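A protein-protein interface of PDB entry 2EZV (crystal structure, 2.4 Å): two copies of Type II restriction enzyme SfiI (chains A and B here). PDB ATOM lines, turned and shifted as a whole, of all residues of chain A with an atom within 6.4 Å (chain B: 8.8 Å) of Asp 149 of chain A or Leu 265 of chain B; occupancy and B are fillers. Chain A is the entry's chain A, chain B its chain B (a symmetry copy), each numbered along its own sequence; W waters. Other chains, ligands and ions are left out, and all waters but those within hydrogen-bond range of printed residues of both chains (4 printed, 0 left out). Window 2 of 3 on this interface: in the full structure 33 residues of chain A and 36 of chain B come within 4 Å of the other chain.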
ATOM      1  N   GLN A   3     -15.140   6.383  26.309  1.00  0.00           N
ATOM      2  CA  GLN A   3     -15.356   7.393  27.322  1.00  0.00           C
ATOM      3  C   GLN A   3     -14.419   7.067  28.493  1.00  0.00           C
ATOM      4  O   GLN A   3     -14.035   7.949  29.259  1.00  0.00           O
ATOM      5  CB  GLN A   3     -16.813   7.376  27.779  1.00  0.00           C
ATOM      6  CG  GLN A   3     -17.800   7.797  26.701  1.00  0.00           C
ATOM      7  CD  GLN A   3     -19.191   8.010  27.261  1.00  0.00           C
ATOM      8  OE1 GLN A   3     -19.837   7.073  27.733  1.00  0.00           O
ATOM      9  NE2 GLN A   3     -19.658   9.258  27.221  1.00  0.00           N
ATOM     10  N   TRP A  85     -14.022  18.042  29.324  1.00  0.00           N
ATOM     11  CA  TRP A  85     -14.103  17.021  28.277  1.00  0.00           C
ATOM     12  C   TRP A  85     -13.068  17.461  27.247  1.00  0.00           C
ATOM     13  O   TRP A  85     -12.949  18.660  26.953  1.00  0.00           O
ATOM     14  CB  TRP A  85     -15.463  16.997  27.577  1.00  0.00           C
ATOM     15  CG  TRP A  85     -16.618  16.572  28.398  1.00  0.00           C
ATOM     16  CD1 TRP A  85     -17.546  17.381  28.988  1.00  0.00           C
ATOM     17  CD2 TRP A  85     -17.045  15.229  28.641  1.00  0.00           C
ATOM     18  NE1 TRP A  85     -18.533  16.625  29.574  1.00  0.00           N
ATOM     19  CE2 TRP A  85     -18.253  15.301  29.376  1.00  0.00           C
ATOM     20  CE3 TRP A  85     -16.530  13.969  28.306  1.00  0.00           C
ATOM     21  CZ2 TRP A  85     -18.953  14.162  29.777  1.00  0.00           C
ATOM     22  CZ3 TRP A  85     -17.227  12.834  28.706  1.00  0.00           C
ATOM     23  CH2 TRP A  85     -18.429  12.938  29.436  1.00  0.00           C
ATOM     24  N   GLN A 145     -19.762  11.112  38.569  1.00  0.00           N
ATOM     25  CA  GLN A 145     -21.058  10.440  38.645  1.00  0.00           C
ATOM     26  C   GLN A 145     -21.927  10.752  37.419  1.00  0.00           C
ATOM     27  O   GLN A 145     -22.347  11.892  37.216  1.00  0.00           O
ATOM     28  CB  GLN A 145     -21.786  10.871  39.927  1.00  0.00           C
ATOM     29  CG  GLN A 145     -23.155  10.229  40.122  1.00  0.00           C
ATOM     30  CD  GLN A 145     -23.088   8.711  40.152  1.00  0.00           C
ATOM     31  OE1 GLN A 145     -22.400   8.121  40.988  1.00  0.00           O
ATOM     32  NE2 GLN A 145     -23.802   8.072  39.237  1.00  0.00           N
ATOM     33  N   SER A 146     -22.197   9.741  36.602  1.00  0.00           N
ATOM     34  CA  SER A 146     -23.023   9.960  35.418  1.00  0.00           C
ATOM     35  C   SER A 146     -24.466  10.137  35.852  1.00  0.00           C
ATOM     36  O   SER A 146     -24.856   9.730  36.949  1.00  0.00           O
ATOM     37  CB  SER A 146     -22.928   8.783  34.447  1.00  0.00           C
ATOM     38  OG  SER A 146     -23.544   7.631  34.983  1.00  0.00           O
ATOM     39  N   ALA A 147     -25.257  10.751  34.991  1.00  0.00           N
ATOM     40  CA  ALA A 147     -26.657  10.976  35.308  1.00  0.00           C
ATOM     41  C   ALA A 147     -27.487   9.731  35.012  1.00  0.00           C
ATOM     42  O   ALA A 147     -28.580   9.576  35.536  1.00  0.00           O
ATOM     43  CB  ALA A 147     -27.179  12.150  34.505  1.00  0.00           C
ATOM     44  N   ASN A 148     -26.959   8.833  34.189  1.00  0.00           N
ATOM     45  CA  ASN A 148     -27.714   7.639  33.820  1.00  0.00           C
ATOM     46  C   ASN A 148     -27.108   6.298  34.223  1.00  0.00           C
ATOM     47  O   ASN A 148     -27.613   5.250  33.817  1.00  0.00           O
ATOM     48  CB  ASN A 148     -27.958   7.651  32.305  1.00  0.00           C
ATOM     49  CG  ASN A 148     -26.663   7.783  31.500  1.00  0.00           C
ATOM     50  OD1 ASN A 148     -25.714   8.430  31.937  1.00  0.00           O
ATOM     51  ND2 ASN A 148     -26.635   7.184  30.313  1.00  0.00           N
ATOM     52  N   ASP A 149     -26.051   6.311  35.031  1.00  0.00           N
ATOM     53  CA  ASP A 149     -25.412   5.057  35.418  1.00  0.00           C
ATOM     54  C   ASP A 149     -24.424   5.181  36.573  1.00  0.00           C
ATOM     55  O   ASP A 149     -24.657   5.901  37.539  1.00  0.00           O
ATOM     56  CB  ASP A 149     -24.718   4.459  34.184  1.00  0.00           C
ATOM     57  CG  ASP A 149     -23.746   3.342  34.528  1.00  0.00           C
ATOM     58  OD1 ASP A 149     -22.532   3.626  34.667  1.00  0.00           O
ATOM     59  OD2 ASP A 149     -24.197   2.181  34.674  1.00  0.00           O
ATOM     60  N   GLY A 150     -23.324   4.449  36.459  1.00  0.00           N
ATOM     61  CA  GLY A 150     -22.293   4.449  37.468  1.00  0.00           C
ATOM     62  C   GLY A 150     -21.293   5.553  37.218  1.00  0.00           C
ATOM     63  O   GLY A 150     -21.616   6.585  36.609  1.00  0.00           O
ATOM     64  N   VAL A 151     -20.069   5.322  37.683  1.00  0.00           N
ATOM     65  CA  VAL A 151     -19.004   6.292  37.555  1.00  0.00           C
ATOM     66  C   VAL A 151     -18.314   6.297  36.199  1.00  0.00           C
ATOM     67  O   VAL A 151     -18.345   5.317  35.458  1.00  0.00           O
ATOM     68  CB  VAL A 151     -17.955   6.090  38.669  1.00  0.00           C
ATOM     69  CG1 VAL A 151     -18.588   6.387  40.020  1.00  0.00           C
ATOM     70  CG2 VAL A 151     -17.413   4.672  38.635  1.00  0.00           C
ATOM     71  N   LEU A 152     -17.707   7.436  35.892  1.00  0.00           N
ATOM     72  CA  LEU A 152     -16.979   7.672  34.651  1.00  0.00           C
ATOM     73  C   LEU A 152     -15.633   8.257  35.065  1.00  0.00           C
ATOM     74  O   LEU A 152     -15.573   9.343  35.630  1.00  0.00           O
ATOM     75  CB  LEU A 152     -17.738   8.685  33.790  1.00  0.00           C
ATOM     76  CG  LEU A 152     -17.114   9.152  32.473  1.00  0.00           C
ATOM     77  CD1 LEU A 152     -16.886   7.972  31.554  1.00  0.00           C
ATOM     78  CD2 LEU A 152     -18.035  10.159  31.813  1.00  0.00           C
ATOM     79  N   ARG B  22     -19.118  14.637  17.702  1.00  0.00           N
ATOM     80  CA  ARG B  22     -19.242  13.923  18.970  1.00  0.00           C
ATOM     81  C   ARG B  22     -19.399  14.874  20.152  1.00  0.00           C
ATOM     82  O   ARG B  22     -20.255  14.668  21.011  1.00  0.00           O
ATOM     83  CB  ARG B  22     -18.024  13.021  19.205  1.00  0.00           C
ATOM     84  CG  ARG B  22     -18.157  12.162  20.449  1.00  0.00           C
ATOM     85  CD  ARG B  22     -19.383  11.250  20.343  1.00  0.00           C
ATOM     86  NE  ARG B  22     -19.638  10.490  21.566  1.00  0.00           N
ATOM     87  CZ  ARG B  22     -20.127  11.015  22.687  1.00  0.00           C
ATOM     88  NH1 ARG B  22     -20.417  12.310  22.746  1.00  0.00           N
ATOM     89  NH2 ARG B  22     -20.340  10.241  23.750  1.00  0.00           N
ATOM     90  N   VAL B  25     -22.811  16.355  20.265  1.00  0.00           N
ATOM     91  CA  VAL B  25     -23.850  15.402  20.673  1.00  0.00           C
ATOM     92  C   VAL B  25     -23.952  15.294  22.188  1.00  0.00           C
ATOM     93  O   VAL B  25     -25.054  15.104  22.713  1.00  0.00           O
ATOM     94  CB  VAL B  25     -23.613  13.986  20.096  1.00  0.00           C
ATOM     95  CG1 VAL B  25     -24.628  12.990  20.694  1.00  0.00           C
ATOM     96  CG2 VAL B  25     -23.766  14.017  18.596  1.00  0.00           C
ATOM     97  N   GLN B  26     -22.818  15.394  22.888  1.00  0.00           N
ATOM     98  CA  GLN B  26     -22.814  15.340  24.352  1.00  0.00           C
ATOM     99  C   GLN B  26     -23.530  16.559  24.892  1.00  0.00           C
ATOM    100  O   GLN B  26     -24.294  16.472  25.848  1.00  0.00           O
ATOM    101  CB  GLN B  26     -21.397  15.372  24.924  1.00  0.00           C
ATOM    102  CG  GLN B  26     -20.711  14.038  24.985  1.00  0.00           C
ATOM    103  CD  GLN B  26     -21.305  13.082  25.998  1.00  0.00           C
ATOM    104  OE1 GLN B  26     -21.318  11.890  25.767  1.00  0.00           O
ATOM    105  NE2 GLN B  26     -21.775  13.595  27.121  1.00  0.00           N
ATOM    106  N   GLN B  29     -27.123  16.180  24.321  1.00  0.00           N
ATOM    107  CA  GLN B  29     -27.591  15.124  25.204  1.00  0.00           C
ATOM    108  C   GLN B  29     -27.794  15.637  26.624  1.00  0.00           C
ATOM    109  O   GLN B  29     -28.881  15.511  27.193  1.00  0.00           O
ATOM    110  CB  GLN B  29     -26.600  13.962  25.238  1.00  0.00           C
ATOM    111  CG  GLN B  29     -26.943  12.926  26.308  1.00  0.00           C
ATOM    112  CD  GLN B  29     -28.299  12.265  26.079  1.00  0.00           C
ATOM    113  OE1 GLN B  29     -28.959  11.837  27.028  1.00  0.00           O
ATOM    114  NE2 GLN B  29     -28.711  12.165  24.816  1.00  0.00           N
ATOM    115  N   GLN B  30     -26.739  16.212  27.189  1.00  0.00           N
ATOM    116  CA  GLN B  30     -26.781  16.722  28.547  1.00  0.00           C
ATOM    117  C   GLN B  30     -27.737  17.902  28.711  1.00  0.00           C
ATOM    118  O   GLN B  30     -28.148  18.232  29.825  1.00  0.00           O
ATOM    119  CB  GLN B  30     -25.353  17.075  28.996  1.00  0.00           C
ATOM    120  CG  GLN B  30     -24.444  15.837  28.986  1.00  0.00           C
ATOM    121  CD  GLN B  30     -23.059  16.053  29.573  1.00  0.00           C
ATOM    122  OE1 GLN B  30     -22.300  15.103  29.737  1.00  0.00           O
ATOM    123  NE2 GLN B  30     -22.725  17.296  29.886  1.00  0.00           N
ATOM    124  N   PRO B 248     -29.209   8.502  25.227  1.00  0.00           N
ATOM    125  CA  PRO B 248     -27.817   8.749  24.843  1.00  0.00           C
ATOM    126  C   PRO B 248     -27.309   7.653  23.909  1.00  0.00           C
ATOM    127  O   PRO B 248     -26.680   6.692  24.349  1.00  0.00           O
ATOM    128  CB  PRO B 248     -27.097   8.748  26.187  1.00  0.00           C
ATOM    129  CG  PRO B 248     -27.862   7.682  26.936  1.00  0.00           C
ATOM    130  CD  PRO B 248     -29.296   8.033  26.624  1.00  0.00           C
ATOM    131  N   ARG B 249     -27.588   7.796  22.621  1.00  0.00           N
ATOM    132  CA  ARG B 249     -27.158   6.805  21.653  1.00  0.00           C
ATOM    133  C   ARG B 249     -26.233   7.423  20.611  1.00  0.00           C
ATOM    134  O   ARG B 249     -26.552   8.445  20.004  1.00  0.00           O
ATOM    135  CB  ARG B 249     -28.385   6.157  20.978  1.00  0.00           C
ATOM    136  N   TRP B 250     -25.071   6.808  20.425  1.00  0.00           N
ATOM    137  CA  TRP B 250     -24.112   7.304  19.448  1.00  0.00           C
ATOM    138  C   TRP B 250     -23.918   6.261  18.373  1.00  0.00           C
ATOM    139  O   TRP B 250     -23.659   5.096  18.669  1.00  0.00           O
ATOM    140  CB  TRP B 250     -22.768   7.637  20.115  1.00  0.00           C
ATOM    141  CG  TRP B 250     -21.635   7.854  19.140  1.00  0.00           C
ATOM    142  CD1 TRP B 250     -20.675   6.951  18.789  1.00  0.00           C
ATOM    143  CD2 TRP B 250     -21.360   9.046  18.382  1.00  0.00           C
ATOM    144  NE1 TRP B 250     -19.817   7.501  17.863  1.00  0.00           N
ATOM    145  CE2 TRP B 250     -20.213   8.783  17.594  1.00  0.00           C
ATOM    146  CE3 TRP B 250     -21.970  10.309  18.294  1.00  0.00           C
ATOM    147  CZ2 TRP B 250     -19.661   9.734  16.727  1.00  0.00           C
ATOM    148  CZ3 TRP B 250     -21.425  11.255  17.433  1.00  0.00           C
ATOM    149  CH2 TRP B 250     -20.278  10.960  16.660  1.00  0.00           C
ATOM    150  N   LYS B 262     -24.138   2.502  20.317  1.00  0.00           N
ATOM    151  CA  LYS B 262     -23.797   2.271  21.698  1.00  0.00           C
ATOM    152  C   LYS B 262     -24.461   3.370  22.495  1.00  0.00           C
ATOM    153  O   LYS B 262     -24.809   4.417  21.949  1.00  0.00           O
ATOM    154  CB  LYS B 262     -22.279   2.362  21.893  1.00  0.00           C
ATOM    155  CG  LYS B 262     -21.690   3.725  21.497  1.00  0.00           C
ATOM    156  CD  LYS B 262     -20.221   3.880  21.880  1.00  0.00           C
ATOM    157  CE  LYS B 262     -20.048   3.989  23.380  1.00  0.00           C
ATOM    158  NZ  LYS B 262     -18.644   4.304  23.773  1.00  0.00           N
ATOM    159  N   GLU B 263     -24.664   3.118  23.780  1.00  0.00           N
ATOM    160  CA  GLU B 263     -25.218   4.129  24.658  1.00  0.00           C
ATOM    161  C   GLU B 263     -24.011   4.662  25.417  1.00  0.00           C
ATOM    162  O   GLU B 263     -23.074   3.923  25.708  1.00  0.00           O
ATOM    163  CB  GLU B 263     -26.251   3.533  25.621  1.00  0.00           C
ATOM    164  CG  GLU B 263     -27.609   3.283  24.958  1.00  0.00           C
ATOM    165  CD  GLU B 263     -28.747   3.130  25.958  1.00  0.00           C
ATOM    166  OE1 GLU B 263     -29.061   4.115  26.666  1.00  0.00           O
ATOM    167  OE2 GLU B 263     -29.325   2.021  26.036  1.00  0.00           O
ATOM    168  N   PHE B 264     -24.019   5.950  25.713  1.00  0.00           N
ATOM    169  CA  PHE B 264     -22.905   6.556  26.418  1.00  0.00           C
ATOM    170  C   PHE B 264     -23.387   7.245  27.673  1.00  0.00           C
ATOM    171  O   PHE B 264     -24.570   7.548  27.814  1.00  0.00           O
ATOM    172  CB  PHE B 264     -22.195   7.548  25.499  1.00  0.00           C
ATOM    173  CG  PHE B 264     -23.074   8.663  25.001  1.00  0.00           C
ATOM    174  CD1 PHE B 264     -23.291   9.800  25.778  1.00  0.00           C
ATOM    175  CD2 PHE B 264     -23.667   8.586  23.748  1.00  0.00           C
ATOM    176  CE1 PHE B 264     -24.085  10.850  25.310  1.00  0.00           C
ATOM    177  CE2 PHE B 264     -24.464   9.626  23.270  1.00  0.00           C
ATOM    178  CZ  PHE B 264     -24.672  10.765  24.055  1.00  0.00           C
ATOM    179  N   LEU B 265     -22.471   7.481  28.599  1.00  0.00           N
ATOM    180  CA  LEU B 265     -22.835   8.136  29.838  1.00  0.00           C
ATOM    181  C   LEU B 265     -22.822   9.639  29.632  1.00  0.00           C
ATOM    182  O   LEU B 265     -22.088  10.151  28.793  1.00  0.00           O
ATOM    183  CB  LEU B 265     -21.848   7.756  30.931  1.00  0.00           C
ATOM    184  CG  LEU B 265     -21.640   6.257  31.138  1.00  0.00           C
ATOM    185  CD1 LEU B 265     -20.627   6.043  32.252  1.00  0.00           C
ATOM    186  CD2 LEU B 265     -22.960   5.594  31.481  1.00  0.00           C
ATOM    187  N   PHE B 266     -23.646  10.344  30.393  1.00  0.00           N
ATOM    188  CA  PHE B 266     -23.696  11.793  30.304  1.00  0.00           C
ATOM    189  C   PHE B 266     -23.909  12.331  31.705  1.00  0.00           C
ATOM    190  O   PHE B 266     -24.388  11.605  32.581  1.00  0.00           O
ATOM    191  CB  PHE B 266     -24.818  12.243  29.353  1.00  0.00           C
ATOM    192  CG  PHE B 266     -26.213  11.910  29.830  1.00  0.00           C
ATOM    193  CD1 PHE B 266     -26.931  12.810  30.610  1.00  0.00           C
ATOM    194  CD2 PHE B 266     -26.824  10.718  29.453  1.00  0.00           C
ATOM    195  CE1 PHE B 266     -28.246  12.529  31.004  1.00  0.00           C
ATOM    196  CE2 PHE B 266     -28.129  10.430  29.840  1.00  0.00           C
ATOM    197  CZ  PHE B 266     -28.842  11.338  30.616  1.00  0.00           C
ATOM    198  N   LEU B 267     -23.537  13.587  31.928  1.00  0.00           N
ATOM    199  CA  LEU B 267     -23.695  14.192  33.242  1.00  0.00           C
ATOM    200  C   LEU B 267     -24.844  15.195  33.259  1.00  0.00           C
ATOM    201  O   LEU B 267     -25.376  15.564  32.212  1.00  0.00           O
ATOM    202  CB  LEU B 267     -22.402  14.909  33.663  1.00  0.00           C
ATOM    203  CG  LEU B 267     -21.073  14.153  33.713  1.00  0.00           C
ATOM    204  CD1 LEU B 267     -21.276  12.755  34.266  1.00  0.00           C
ATOM    205  CD2 LEU B 267     -20.512  14.060  32.336  1.00  0.00           C
ATOM    206  N   GLU B 268     -25.212  15.641  34.456  1.00  0.00           N
ATOM    207  CA  GLU B 268     -26.276  16.620  34.621  1.00  0.00           C
ATOM    208  C   GLU B 268     -25.822  17.991  34.109  1.00  0.00           C
ATOM    209  O   GLU B 268     -26.609  18.744  33.537  1.00  0.00           O
ATOM    210  CB  GLU B 268     -26.666  16.719  36.092  1.00  0.00           C
HETATM  211  O   HOH W   1     -28.783   5.587  29.611  1.00  0.00           O
HETATM  212  O   HOH W   2     -24.185  13.720  36.709  1.00  0.00           O
HETATM  213  O   HOH W   3     -17.959  11.078  25.855  1.00  0.00           O
HETATM  214  O   HOH W   4     -20.293  18.802  30.775  1.00  0.00           O
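The backbone NH (N) of Leu 265 of chain B lies within hydrogen-bond range of the side-chain amide oxygen (OE1) of Gln 3 of chain A (2.8 Å).
The side-chain amide oxygen (OE1) of Gln 26 of chain B lies within hydrogen-bond range of the side-chain amide nitrogen (NE2) of Gln 3 of chain A (3.4 Å).
The backbone carbonyl oxygen (O) of Phe 266 of chain B is in hydrogen-bond range of the backbone NH (N) of Ala 147 of chain A (2.7 Å).
The backbone NH of Phe 266 of chain B is in hydrogen-bond range of the side-chain amide oxygen of Asn 148 of chain A (3.2 Å).
ND2 of Asn 148 of chain A is in hydrogen-bond range of O of Phe 264 of chain B.
The backbone carbonyl oxygen (O) of Pro 248 of chain B is in hydrogen-bond range of the backbone NH (N) of Phe 264 of chain B (3.1 Å).
The side-chain hydroxyl (OG) of Ser 146 of chain A lies within hydrogen-bond range of the backbone carbonyl oxygen (O) of Gly 150 of chain A, 2.7 Å away.
N of Asp 149 of chain A lies within hydrogen-bond range of OG of Ser 146 of chain A, at 2.8 Å.
The guanidinium group (NH2) of Arg 22 of chain B is in hydrogen-bond range of the side-chain amide oxygen (OE1) of Gln 26 of chain B (2.8 Å).
OE1 of Gln 30 of chain B lies within hydrogen-bond range of N of Leu 267 of chain B (2.9 Å).
NE2 of Gln 26 of chain B is in hydrogen-bond range of OE1 of Gln 30 of chain B (3.1 Å).
Among the printed residues, merely in contact across the chains: Gln 3 of chain A with Arg 22 of chain B (3.7 Å), Gln 3 of chain A with Phe 264 of chain B (3.3 Å), Trp 85 of chain A with Gln 26 of chain B (3.9 Å), Trp 85 of chain A with Gln 30 of chain B (3.5 Å), Trp 85 of chain A with Leu 267 of chain B (3.0 Å), Gln 145 of chain A with Leu 267 of chain B (3.3 Å), Ser 146 of chain A with Leu 265 of chain B (3.8 Å), Ser 146 of chain A with Phe 266 of chain B (3.6 Å), Ser 146 of chain A with Leu 267 of chain B (3.5 Å), Asn 148 of chain A with Pro 248 of chain B (3.6 Å), Asn 148 of chain A with Leu 265 of chain B (3.6 Å) and Asp 149 of chain A with Leu 265 of chain B (3.4 Å).
Asp 149 of chain A touches one residue of chain B.
Printed residues of chain A within 4 Å of Leu 265 of chain B: Gln 3, Ser 146, Asn 148 and Asp 149.
Of the printed residues of chain A, Gln 26 of chain B touches Gln 3 (3.4 Å) and Trp 85 (3.9 Å).
Printed residues of chain B within 4 Å of Gln 145 of chain A: Leu 267 (3.3 Å).
Printed residues of chain A within 4 Å of Gln 30 of chain B: Trp 85 (3.5 Å).
Val 151 of chain A touches none of the printed residues of chain B.
The nearest residue of chain B that does not touch Asp 149 of chain A is Phe 266 of chain B (6.1 Å).
Of the 10 printed residues of chain A, 7 touch a printed residue of chain B.
Printed residues of chain B that touch a printed residue of chain A: Arg 22, Gln 26, Gln 30, Pro 248, Phe 264, Leu 265, Phe 266 and Leu 267.
Hydrophobic or aromatic side chains of chain B that line the printed part of chain A: Pro 248, Phe 264, Leu 265, Phe 266 and Leu 267.
Among the printed residues, 17 pairs touch across the chains.
Among the printed residues, no Asp or Glu carboxylate lies within 4 Å of a Lys or Arg side-chain nitrogen of the other chain.
No position is printed for both chains.
Water W2 bridges O of Gln 145 of chain A (2.6 Å) and N of Glu 268 of chain B (3.1 Å).
Water W1 lies within hydrogen-bond range of ND2 of Asn 148 of chain A and OE1 of Glu 263 of chain B.
Water W3 lies within hydrogen-bond range of NE2 of Gln 3 of chain A (2.8 Å), NH2 of Arg 22 of chain B (3.3 Å) and OE1 of Gln 26 of chain B (3.5 Å).
Water W4 lies within hydrogen-bond range of NE2 of Gln 30 of chain B (3.0 Å) and NE1 of Trp 85 of chain A (3.0 Å).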
